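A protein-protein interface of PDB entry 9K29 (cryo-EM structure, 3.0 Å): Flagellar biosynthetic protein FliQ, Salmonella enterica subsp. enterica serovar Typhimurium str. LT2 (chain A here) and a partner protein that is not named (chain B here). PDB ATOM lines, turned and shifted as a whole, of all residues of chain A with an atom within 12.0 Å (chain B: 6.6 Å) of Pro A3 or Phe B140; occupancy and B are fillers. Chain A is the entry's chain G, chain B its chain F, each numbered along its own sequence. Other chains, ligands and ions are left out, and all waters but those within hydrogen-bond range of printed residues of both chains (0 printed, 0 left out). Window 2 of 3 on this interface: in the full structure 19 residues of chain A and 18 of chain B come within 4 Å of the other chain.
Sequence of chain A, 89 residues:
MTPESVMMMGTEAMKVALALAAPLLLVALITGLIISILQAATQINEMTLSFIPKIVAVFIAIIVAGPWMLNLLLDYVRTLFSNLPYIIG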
ATOM      1  N   MET A   1       1.905 -21.513   9.933  1.00  0.00           N
ATOM      2  CA  MET A   1       1.288 -21.309   8.629  1.00  0.00           C
ATOM      3  C   MET A   1       2.103 -22.072   7.585  1.00  0.00           C
ATOM      4  O   MET A   1       2.951 -21.505   6.895  1.00  0.00           O
ATOM      5  CB  MET A   1       1.207 -19.813   8.303  1.00  0.00           C
ATOM      6  CG  MET A   1       0.719 -19.456   6.903  1.00  0.00           C
ATOM      7  SD  MET A   1      -1.046 -19.754   6.695  1.00  0.00           S
ATOM      8  CE  MET A   1      -1.499 -18.383   5.636  1.00  0.00           C
ATOM      9  N   THR A   2       1.863 -23.377   7.505  1.00  0.00           N
ATOM     10  CA  THR A   2       2.590 -24.215   6.569  1.00  0.00           C
ATOM     11  C   THR A   2       2.068 -23.993   5.148  1.00  0.00           C
ATOM     12  O   THR A   2       0.919 -23.583   4.959  1.00  0.00           O
ATOM     13  CB  THR A   2       2.458 -25.688   6.963  1.00  0.00           C
ATOM     14  OG1 THR A   2       3.271 -26.501   6.109  1.00  0.00           O
ATOM     15  CG2 THR A   2       1.012 -26.148   6.869  1.00  0.00           C
ATOM     16  N   PRO A   3       2.903 -24.228   4.132  1.00  0.00           N
ATOM     17  CA  PRO A   3       2.409 -24.119   2.750  1.00  0.00           C
ATOM     18  C   PRO A   3       1.223 -25.018   2.461  1.00  0.00           C
ATOM     19  O   PRO A   3       0.332 -24.623   1.699  1.00  0.00           O
ATOM     20  CB  PRO A   3       3.633 -24.510   1.912  1.00  0.00           C
ATOM     21  CG  PRO A   3       4.791 -24.140   2.762  1.00  0.00           C
ATOM     22  CD  PRO A   3       4.367 -24.382   4.182  1.00  0.00           C
ATOM     23  N   GLU A   4       1.176 -26.213   3.057  1.00  0.00           N
ATOM     24  CA  GLU A   4       0.031 -27.095   2.854  1.00  0.00           C
ATOM     25  C   GLU A   4      -1.257 -26.452   3.353  1.00  0.00           C
ATOM     26  O   GLU A   4      -2.326 -26.657   2.769  1.00  0.00           O
ATOM     27  CB  GLU A   4       0.266 -28.437   3.549  1.00  0.00           C
ATOM     28  CG  GLU A   4       1.322 -29.311   2.889  1.00  0.00           C
ATOM     29  CD  GLU A   4       2.736 -28.898   3.244  1.00  0.00           C
ATOM     30  OE1 GLU A   4       3.007 -28.671   4.440  1.00  0.00           O
ATOM     31  OE2 GLU A   4       3.576 -28.801   2.325  1.00  0.00           O
ATOM     32  N   SER A   5      -1.179 -25.679   4.439  1.00  0.00           N
ATOM     33  CA  SER A   5      -2.362 -24.982   4.932  1.00  0.00           C
ATOM     34  C   SER A   5      -2.868 -23.969   3.914  1.00  0.00           C
ATOM     35  O   SER A   5      -4.075 -23.883   3.659  1.00  0.00           O
ATOM     36  CB  SER A   5      -2.054 -24.298   6.263  1.00  0.00           C
ATOM     37  OG  SER A   5      -1.261 -23.141   6.067  1.00  0.00           O
ATOM     38  N   VAL A   6      -1.958 -23.199   3.313  1.00  0.00           N
ATOM     39  CA  VAL A   6      -2.349 -22.244   2.279  1.00  0.00           C
ATOM     40  C   VAL A   6      -2.953 -22.974   1.089  1.00  0.00           C
ATOM     41  O   VAL A   6      -3.934 -22.518   0.487  1.00  0.00           O
ATOM     42  CB  VAL A   6      -1.138 -21.391   1.857  1.00  0.00           C
ATOM     43  CG1 VAL A   6      -1.534 -20.397   0.777  1.00  0.00           C
ATOM     44  CG2 VAL A   6      -0.541 -20.685   3.058  1.00  0.00           C
ATOM     45  N   MET A   7      -2.368 -24.114   0.728  1.00  0.00           N
ATOM     46  CA  MET A   7      -2.837 -24.865  -0.429  1.00  0.00           C
ATOM     47  C   MET A   7      -4.248 -25.393  -0.192  1.00  0.00           C
ATOM     48  O   MET A   7      -5.118 -25.299  -1.070  1.00  0.00           O
ATOM     49  CB  MET A   7      -1.864 -26.009  -0.694  1.00  0.00           C
ATOM     50  CG  MET A   7      -0.480 -25.520  -1.091  1.00  0.00           C
ATOM     51  SD  MET A   7      -0.437 -24.545  -2.588  1.00  0.00           S
ATOM     52  CE  MET A   7      -0.814 -25.853  -3.717  1.00  0.00           C
ATOM     53  N   MET A   8      -4.489 -25.939   1.003  1.00  0.00           N
ATOM     54  CA  MET A   8      -5.818 -26.415   1.367  1.00  0.00           C
ATOM     55  C   MET A   8      -6.812 -25.264   1.425  1.00  0.00           C
ATOM     56  O   MET A   8      -7.973 -25.418   1.031  1.00  0.00           O
ATOM     57  CB  MET A   8      -5.752 -27.159   2.703  1.00  0.00           C
ATOM     58  CG  MET A   8      -7.064 -27.776   3.182  1.00  0.00           C
ATOM     59  SD  MET A   8      -8.188 -26.637   4.016  1.00  0.00           S
ATOM     60  CE  MET A   8      -7.332 -26.398   5.570  1.00  0.00           C
ATOM     61  N   MET A   9      -6.376 -24.103   1.919  1.00  0.00           N
ATOM     62  CA  MET A   9      -7.243 -22.931   1.934  1.00  0.00           C
ATOM     63  C   MET A   9      -7.650 -22.535   0.521  1.00  0.00           C
ATOM     64  O   MET A   9      -8.819 -22.225   0.267  1.00  0.00           O
ATOM     65  CB  MET A   9      -6.534 -21.778   2.650  1.00  0.00           C
ATOM     66  CG  MET A   9      -7.344 -20.496   2.804  1.00  0.00           C
ATOM     67  SD  MET A   9      -7.344 -19.433   1.347  1.00  0.00           S
ATOM     68  CE  MET A   9      -5.670 -18.799   1.394  1.00  0.00           C
ATOM     69  N   GLY A  10      -6.700 -22.549  -0.414  1.00  0.00           N
ATOM     70  CA  GLY A  10      -7.031 -22.231  -1.794  1.00  0.00           C
ATOM     71  C   GLY A  10      -7.987 -23.234  -2.416  1.00  0.00           C
ATOM     72  O   GLY A  10      -8.929 -22.857  -3.123  1.00  0.00           O
ATOM     73  N   THR A  11      -7.755 -24.526  -2.167  1.00  0.00           N
ATOM     74  CA  THR A  11      -8.653 -25.545  -2.703  1.00  0.00           C
ATOM     75  C   THR A  11     -10.058 -25.397  -2.131  1.00  0.00           C
ATOM     76  O   THR A  11     -11.049 -25.523  -2.859  1.00  0.00           O
ATOM     77  CB  THR A  11      -8.109 -26.944  -2.419  1.00  0.00           C
ATOM     78  OG1 THR A  11      -7.748 -27.047  -1.037  1.00  0.00           O
ATOM     79  CG2 THR A  11      -6.889 -27.224  -3.279  1.00  0.00           C
ATOM     80  N   GLU A  12     -10.163 -25.130  -0.827  1.00  0.00           N
ATOM     81  CA  GLU A  12     -11.467 -24.912  -0.211  1.00  0.00           C
ATOM     82  C   GLU A  12     -12.147 -23.677  -0.787  1.00  0.00           C
ATOM     83  O   GLU A  12     -13.365 -23.672  -1.007  1.00  0.00           O
ATOM     84  CB  GLU A  12     -11.315 -24.784   1.303  1.00  0.00           C
ATOM     85  CG  GLU A  12     -12.599 -24.433   2.034  1.00  0.00           C
ATOM     86  CD  GLU A  12     -13.402 -25.655   2.432  1.00  0.00           C
ATOM     87  OE1 GLU A  12     -12.969 -26.783   2.117  1.00  0.00           O
ATOM     88  OE2 GLU A  12     -14.468 -25.485   3.061  1.00  0.00           O
ATOM     89  N   TYR A  86      -6.012 -19.477  14.767  1.00  0.00           N
ATOM     90  CA  TYR A  86      -5.307 -20.754  14.812  1.00  0.00           C
ATOM     91  C   TYR A  86      -4.277 -20.876  13.697  1.00  0.00           C
ATOM     92  O   TYR A  86      -3.266 -21.569  13.864  1.00  0.00           O
ATOM     93  CB  TYR A  86      -6.307 -21.908  14.736  1.00  0.00           C
ATOM     94  CG  TYR A  86      -7.188 -22.040  15.958  1.00  0.00           C
ATOM     95  CD1 TYR A  86      -6.876 -21.381  17.140  1.00  0.00           C
ATOM     96  CD2 TYR A  86      -8.333 -22.825  15.930  1.00  0.00           C
ATOM     97  CE1 TYR A  86      -7.679 -21.499  18.257  1.00  0.00           C
ATOM     98  CE2 TYR A  86      -9.143 -22.949  17.042  1.00  0.00           C
ATOM     99  CZ  TYR A  86      -8.811 -22.284  18.203  1.00  0.00           C
ATOM    100  OH  TYR A  86      -9.613 -22.404  19.314  1.00  0.00           O
ATOM    101  N   ILE A  87      -4.508 -20.220  12.559  1.00  0.00           N
ATOM    102  CA  ILE A  87      -3.593 -20.350  11.430  1.00  0.00           C
ATOM    103  C   ILE A  87      -2.360 -19.469  11.582  1.00  0.00           C
ATOM    104  O   ILE A  87      -1.372 -19.670  10.864  1.00  0.00           O
ATOM    105  CB  ILE A  87      -4.320 -20.031  10.112  1.00  0.00           C
ATOM    106  CG1 ILE A  87      -3.645 -20.747   8.941  1.00  0.00           C
ATOM    107  CG2 ILE A  87      -4.356 -18.529   9.868  1.00  0.00           C
ATOM    108  CD1 ILE A  87      -3.760 -22.255   9.001  1.00  0.00           C
ATOM    109  N   ILE A  88      -2.383 -18.502  12.500  1.00  0.00           N
ATOM    110  CA  ILE A  88      -1.246 -17.610  12.679  1.00  0.00           C
ATOM    111  C   ILE A  88      -0.138 -18.330  13.434  1.00  0.00           C
ATOM    112  O   ILE A  88      -0.373 -18.958  14.476  1.00  0.00           O
ATOM    113  CB  ILE A  88      -1.682 -16.332  13.413  1.00  0.00           C
ATOM    114  CG1 ILE A  88      -2.718 -15.575  12.585  1.00  0.00           C
ATOM    115  CG2 ILE A  88      -0.482 -15.445  13.707  1.00  0.00           C
ATOM    116  CD1 ILE A  88      -3.379 -14.448  13.333  1.00  0.00           C
ATOM    117  N   GLY A  89       1.081 -18.243  12.909  1.00  0.00           N
ATOM    118  CA  GLY A  89       2.230 -18.860  13.543  1.00  0.00           C
ATOM    119  C   GLY A  89       3.023 -17.899  14.407  1.00  0.00           C
ATOM    120  O   GLY A  89       3.792 -18.311  15.275  1.00  0.00           O
ATOM    121  OXT GLY A  89       2.918 -16.681  14.261  1.00  0.00           O
ATOM    122  N   ALA B 133       0.510 -16.975  -4.528  1.00  0.00           N
ATOM    123  CA  ALA B 133       1.949 -16.812  -4.693  1.00  0.00           C
ATOM    124  C   ALA B 133       2.544 -15.968  -3.572  1.00  0.00           C
ATOM    125  O   ALA B 133       3.612 -16.292  -3.046  1.00  0.00           O
ATOM    126  CB  ALA B 133       2.251 -16.192  -6.056  1.00  0.00           C
ATOM    127  N   LEU B 135       1.314 -15.563  -0.507  1.00  0.00           N
ATOM    128  CA  LEU B 135       1.261 -16.326   0.735  1.00  0.00           C
ATOM    129  C   LEU B 135       2.360 -17.380   0.776  1.00  0.00           C
ATOM    130  O   LEU B 135       2.979 -17.603   1.824  1.00  0.00           O
ATOM    131  CB  LEU B 135      -0.114 -16.968   0.904  1.00  0.00           C
ATOM    132  CG  LEU B 135      -1.213 -16.037   1.418  1.00  0.00           C
ATOM    133  CD1 LEU B 135      -2.583 -16.670   1.244  1.00  0.00           C
ATOM    134  CD2 LEU B 135      -0.966 -15.675   2.871  1.00  0.00           C
ATOM    135  N   LEU B 136       2.620 -18.038  -0.355  1.00  0.00           N
ATOM    136  CA  LEU B 136       3.735 -18.978  -0.415  1.00  0.00           C
ATOM    137  C   LEU B 136       5.064 -18.258  -0.218  1.00  0.00           C
ATOM    138  O   LEU B 136       5.968 -18.777   0.448  1.00  0.00           O
ATOM    139  CB  LEU B 136       3.711 -19.731  -1.743  1.00  0.00           C
ATOM    140  CG  LEU B 136       2.551 -20.717  -1.903  1.00  0.00           C
ATOM    141  CD1 LEU B 136       2.830 -21.705  -3.018  1.00  0.00           C
ATOM    142  CD2 LEU B 136       2.273 -21.446  -0.598  1.00  0.00           C
ATOM    143  N   PHE B 137       5.196 -17.059  -0.787  1.00  0.00           N
ATOM    144  CA  PHE B 137       6.385 -16.243  -0.572  1.00  0.00           C
ATOM    145  C   PHE B 137       6.586 -15.953   0.909  1.00  0.00           C
ATOM    146  O   PHE B 137       7.711 -16.020   1.418  1.00  0.00           O
ATOM    147  CB  PHE B 137       6.254 -14.938  -1.361  1.00  0.00           C
ATOM    148  CG  PHE B 137       7.555 -14.235  -1.607  1.00  0.00           C
ATOM    149  CD1 PHE B 137       8.623 -14.902  -2.179  1.00  0.00           C
ATOM    150  CD2 PHE B 137       7.705 -12.900  -1.276  1.00  0.00           C
ATOM    151  CE1 PHE B 137       9.817 -14.252  -2.413  1.00  0.00           C
ATOM    152  CE2 PHE B 137       8.898 -12.245  -1.504  1.00  0.00           C
ATOM    153  CZ  PHE B 137       9.954 -12.922  -2.075  1.00  0.00           C
ATOM    154  N   LEU B 138       5.503 -15.620   1.611  1.00  0.00           N
ATOM    155  CA  LEU B 138       5.586 -15.392   3.050  1.00  0.00           C
ATOM    156  C   LEU B 138       6.001 -16.658   3.790  1.00  0.00           C
ATOM    157  O   LEU B 138       6.859 -16.613   4.679  1.00  0.00           O
ATOM    158  CB  LEU B 138       4.245 -14.888   3.579  1.00  0.00           C
ATOM    159  CG  LEU B 138       3.815 -13.504   3.106  1.00  0.00           C
ATOM    160  CD1 LEU B 138       2.712 -12.961   3.994  1.00  0.00           C
ATOM    161  CD2 LEU B 138       5.006 -12.577   3.104  1.00  0.00           C
ATOM    162  N   THR B 139       5.397 -17.797   3.440  1.00  0.00           N
ATOM    163  CA  THR B 139       5.727 -19.043   4.127  1.00  0.00           C
ATOM    164  C   THR B 139       7.165 -19.473   3.861  1.00  0.00           C
ATOM    165  O   THR B 139       7.759 -20.180   4.682  1.00  0.00           O
ATOM    166  CB  THR B 139       4.763 -20.155   3.714  1.00  0.00           C
ATOM    167  OG1 THR B 139       4.856 -20.374   2.302  1.00  0.00           O
ATOM    168  CG2 THR B 139       3.335 -19.790   4.084  1.00  0.00           C
ATOM    169  N   PHE B 140       7.734 -19.066   2.731  1.00  0.00           N
ATOM    170  CA  PHE B 140       9.118 -19.387   2.405  1.00  0.00           C
ATOM    171  C   PHE B 140      10.098 -18.322   2.876  1.00  0.00           C
ATOM    172  O   PHE B 140      11.296 -18.443   2.603  1.00  0.00           O
ATOM    173  CB  PHE B 140       9.272 -19.599   0.896  1.00  0.00           C
ATOM    174  CG  PHE B 140       8.415 -20.704   0.351  1.00  0.00           C
ATOM    175  CD1 PHE B 140       8.110 -21.807   1.129  1.00  0.00           C
ATOM    176  CD2 PHE B 140       7.915 -20.641  -0.938  1.00  0.00           C
ATOM    177  CE1 PHE B 140       7.320 -22.823   0.635  1.00  0.00           C
ATOM    178  CE2 PHE B 140       7.124 -21.655  -1.437  1.00  0.00           C
ATOM    179  CZ  PHE B 140       6.825 -22.746  -0.648  1.00  0.00           C
ATOM    180  N   ASN B 141       9.617 -17.290   3.573  1.00  0.00           N
ATOM    181  CA  ASN B 141      10.462 -16.210   4.086  1.00  0.00           C
ATOM    182  C   ASN B 141      11.254 -15.542   2.966  1.00  0.00           C
ATOM    183  O   ASN B 141      12.454 -15.290   3.093  1.00  0.00           O
ATOM    184  CB  ASN B 141      11.396 -16.714   5.188  1.00  0.00           C
ATOM    185  CG  ASN B 141      10.665 -17.001   6.483  1.00  0.00           C
ATOM    186  OD1 ASN B 141       9.603 -16.437   6.748  1.00  0.00           O
ATOM    187  ND2 ASN B 141      11.231 -17.881   7.299  1.00  0.00           N
ATOM    188  N   GLY B 142      10.576 -15.261   1.852  1.00  0.00           N
ATOM    189  CA  GLY B 142      11.244 -14.609   0.738  1.00  0.00           C
ATOM    190  C   GLY B 142      11.675 -13.190   1.056  1.00  0.00           C
ATOM    191  O   GLY B 142      12.723 -12.732   0.595  1.00  0.00           O
ATOM    192  N   HIS B 143      10.866 -12.468   1.836  1.00  0.00           N
ATOM    193  CA  HIS B 143      11.231 -11.109   2.226  1.00  0.00           C
ATOM    194  C   HIS B 143      12.493 -11.097   3.081  1.00  0.00           C
ATOM    195  O   HIS B 143      13.336 -10.202   2.946  1.00  0.00           O
ATOM    196  CB  HIS B 143      10.064 -10.447   2.956  1.00  0.00           C
ATOM    197  CG  HIS B 143       9.507 -11.268   4.076  1.00  0.00           C
ATOM    198  ND1 HIS B 143      10.005 -11.214   5.361  1.00  0.00           N
ATOM    199  CD2 HIS B 143       8.493 -12.164   4.104  1.00  0.00           C
ATOM    200  CE1 HIS B 143       9.320 -12.042   6.130  1.00  0.00           C
ATOM    201  NE2 HIS B 143       8.397 -12.630   5.391  1.00  0.00           N
ATOM    202  N   LEU B 144      12.641 -12.084   3.968  1.00  0.00           N
ATOM    203  CA  LEU B 144      13.873 -12.198   4.743  1.00  0.00           C
ATOM    204  C   LEU B 144      15.075 -12.394   3.832  1.00  0.00           C
ATOM    205  O   LEU B 144      16.139 -11.798   4.049  1.00  0.00           O
ATOM    206  CB  LEU B 144      13.763 -13.357   5.733  1.00  0.00           C
ATOM    207  CG  LEU B 144      12.629 -13.300   6.752  1.00  0.00           C
ATOM    208  CD1 LEU B 144      12.791 -14.411   7.773  1.00  0.00           C
ATOM    209  CD2 LEU B 144      12.602 -11.946   7.432  1.00  0.00           C
ATOM    210  N   TRP B 145      14.926 -13.233   2.806  1.00  0.00           N
ATOM    211  CA  TRP B 145      16.016 -13.448   1.864  1.00  0.00           C
ATOM    212  C   TRP B 145      16.324 -12.176   1.085  1.00  0.00           C
ATOM    213  O   TRP B 145      17.489 -11.888   0.792  1.00  0.00           O
ATOM    214  CB  TRP B 145      15.673 -14.596   0.920  1.00  0.00           C
ATOM    215  CG  TRP B 145      15.704 -15.943   1.572  1.00  0.00           C
ATOM    216  CD1 TRP B 145      16.391 -16.296   2.695  1.00  0.00           C
ATOM    217  CD2 TRP B 145      15.018 -17.121   1.134  1.00  0.00           C
ATOM    218  NE1 TRP B 145      16.172 -17.621   2.988  1.00  0.00           N
ATOM    219  CE2 TRP B 145      15.333 -18.150   2.043  1.00  0.00           C
ATOM    220  CE3 TRP B 145      14.167 -17.406   0.061  1.00  0.00           C
ATOM    221  CZ2 TRP B 145      14.828 -19.442   1.912  1.00  0.00           C
ATOM    222  CZ3 TRP B 145      13.667 -18.688  -0.067  1.00  0.00           C
ATOM    223  CH2 TRP B 145      13.998 -19.690   0.853  1.00  0.00           C
ATOM    224  N   ALA B 237       2.136 -25.225  -5.305  1.00  0.00           N
ATOM    225  CA  ALA B 237       3.155 -25.185  -4.256  1.00  0.00           C
ATOM    226  C   ALA B 237       4.561 -25.501  -4.755  1.00  0.00           C
ATOM    227  O   ALA B 237       5.477 -24.707  -4.478  1.00  0.00           O
ATOM    228  CB  ALA B 237       2.751 -26.116  -3.108  1.00  0.00           C
ATOM    229  N   PRO B 238       4.820 -26.607  -5.481  1.00  0.00           N
ATOM    230  CA  PRO B 238       6.196 -26.858  -5.933  1.00  0.00           C
ATOM    231  C   PRO B 238       6.631 -25.898  -7.029  1.00  0.00           C
ATOM    232  O   PRO B 238       7.815 -25.557  -7.146  1.00  0.00           O
ATOM    233  CB  PRO B 238       6.142 -28.304  -6.435  1.00  0.00           C
ATOM    234  CG  PRO B 238       4.741 -28.487  -6.873  1.00  0.00           C
ATOM    235  CD  PRO B 238       3.902 -27.673  -5.928  1.00  0.00           C
ATOM    236  N   CYS B 240       5.852 -22.710  -7.251  1.00  0.00           N
ATOM    237  CA  CYS B 240       6.325 -21.490  -6.605  1.00  0.00           C
ATOM    238  C   CYS B 240       7.687 -21.700  -5.957  1.00  0.00           C
ATOM    239  O   CYS B 240       8.539 -20.804  -5.981  1.00  0.00           O
ATOM    240  CB  CYS B 240       5.305 -21.011  -5.576  1.00  0.00           C
ATOM    241  SG  CYS B 240       3.810 -20.295  -6.294  1.00  0.00           S
ATOM    242  N   GLU B 241       7.911 -22.878  -5.366  1.00  0.00           N
ATOM    243  CA  GLU B 241       9.219 -23.181  -4.796  1.00  0.00           C
ATOM    244  C   GLU B 241      10.309 -23.074  -5.850  1.00  0.00           C
ATOM    245  O   GLU B 241      11.362 -22.473  -5.613  1.00  0.00           O
ATOM    246  CB  GLU B 241       9.221 -24.581  -4.182  1.00  0.00           C
ATOM    247  CG  GLU B 241       8.338 -24.739  -2.963  1.00  0.00           C
ATOM    248  CD  GLU B 241       8.362 -26.149  -2.406  1.00  0.00           C
ATOM    249  OE1 GLU B 241       8.970 -27.031  -3.047  1.00  0.00           O
ATOM    250  OE2 GLU B 241       7.771 -26.375  -1.329  1.00  0.00           O
ATOM    251  N   PHE B 244      10.516 -19.014  -7.159  1.00  0.00           N
ATOM    252  CA  PHE B 244      11.250 -18.096  -6.292  1.00  0.00           C
ATOM    253  C   PHE B 244      12.723 -18.480  -6.204  1.00  0.00           C
ATOM    254  O   PHE B 244      13.599 -17.609  -6.188  1.00  0.00           O
ATOM    255  CB  PHE B 244      10.622 -18.045  -4.897  1.00  0.00           C
ATOM    256  CG  PHE B 244       9.165 -17.682  -4.895  1.00  0.00           C
ATOM    257  CD1 PHE B 244       8.716 -16.561  -5.572  1.00  0.00           C
ATOM    258  CD2 PHE B 244       8.248 -18.436  -4.181  1.00  0.00           C
ATOM    259  CE1 PHE B 244       7.378 -16.218  -5.564  1.00  0.00           C
ATOM    260  CE2 PHE B 244       6.911 -18.096  -4.169  1.00  0.00           C
ATOM    261  CZ  PHE B 244       6.475 -16.986  -4.860  1.00  0.00           C
ATOM    262  N   PHE B 248      15.927 -16.151  -7.107  1.00  0.00           N
ATOM    263  CA  PHE B 248      16.904 -15.841  -6.067  1.00  0.00           C
ATOM    264  C   PHE B 248      18.318 -16.177  -6.525  1.00  0.00           C
ATOM    265  O   PHE B 248      19.260 -15.412  -6.290  1.00  0.00           O
ATOM    266  CB  PHE B 248      16.554 -16.595  -4.785  1.00  0.00           C
ATOM    267  CG  PHE B 248      15.678 -15.818  -3.848  1.00  0.00           C
ATOM    268  CD1 PHE B 248      16.139 -14.656  -3.255  1.00  0.00           C
ATOM    269  CD2 PHE B 248      14.390 -16.241  -3.569  1.00  0.00           C
ATOM    270  CE1 PHE B 248      15.335 -13.936  -2.395  1.00  0.00           C
ATOM    271  CE2 PHE B 248      13.579 -15.523  -2.714  1.00  0.00           C
ATOM    272  CZ  PHE B 248      14.052 -14.371  -2.124  1.00  0.00           C
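The side-chain hydroxyl (OG) of Ser A5 is in hydrogen-bond range of the side-chain sulfur (SD) of Met A1 (3.5 Å).
The backbone carbonyl oxygen of Leu B136 is in hydrogen-bond range of the side-chain hydroxyl of Thr B139, at 2.7 Å.
OG1 of Thr B139 lies close to O of Leu B135, 3.4 Å away.
The backbone carbonyl oxygen (O) of Met A7 lies within hydrogen-bond range of the side-chain hydroxyl (OG1) of Thr A11 (3.2 Å).
Among the printed residues, merely in contact across the chains: Met A1 with Leu B135, Met A1 with Thr B139, Pro A3 with Thr B139, Pro A3 with Phe B140, Val A6 with Leu B135, Met A7 with Ala B237 and Met A9 with Leu B135.
Of the 16 printed residues of chain A, 5 touch a printed residue of chain B.
Printed residues of chain A that touch a printed residue of chain B: Met A1, Pro A3, Val A6, Met A7 and Met A9.
Hydrophobic or aromatic side chains of chain A that line the printed part of chain B: Met A1, Pro A3, Val A6, Met A7 and Met A9.
Hydrophobic or aromatic side chains of chain B within 4 Å of the printed part of chain A: Leu B135, Phe B140 and Ala B237.
Among the printed residues, 7 pairs touch across the chains.
Among the printed residues, no Asp or Glu carboxylate lies within 4 Å of a Lys or Arg side-chain nitrogen of the other chain.
Pro A3 touches just these residues of chain B: Thr B139 and Phe B140.
Printed residues of chain B within 4 Å of Val A6: Leu B135.
Of the printed residues of chain A, Leu B135 touches Met A1, Val A6 and Met A9.
Leu B136 touches none of the printed residues of chain A.
No residue of chain A comes within 4 Å of Phe B137.
Phe B140 touches just one residue of chain A: Pro A3 (3.6 Å).
No residue of chain A comes within 4 Å of Asn B141.
Trp B145 touches none of the printed residues of chain A.
Ala B237 touches one residue of chain A.
Pro B238 touches none of the printed residues of chain A.
Cys B240 touches none of the printed residues of chain A.
No residue of chain A comes within 4 Å of Glu B241.
The nearest residue of chain B that does not touch Pro A3 is Leu B136 (4.2 Å).
The nearest residue of chain A that does not touch Phe B140 is Met A1 (6.8 Å).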
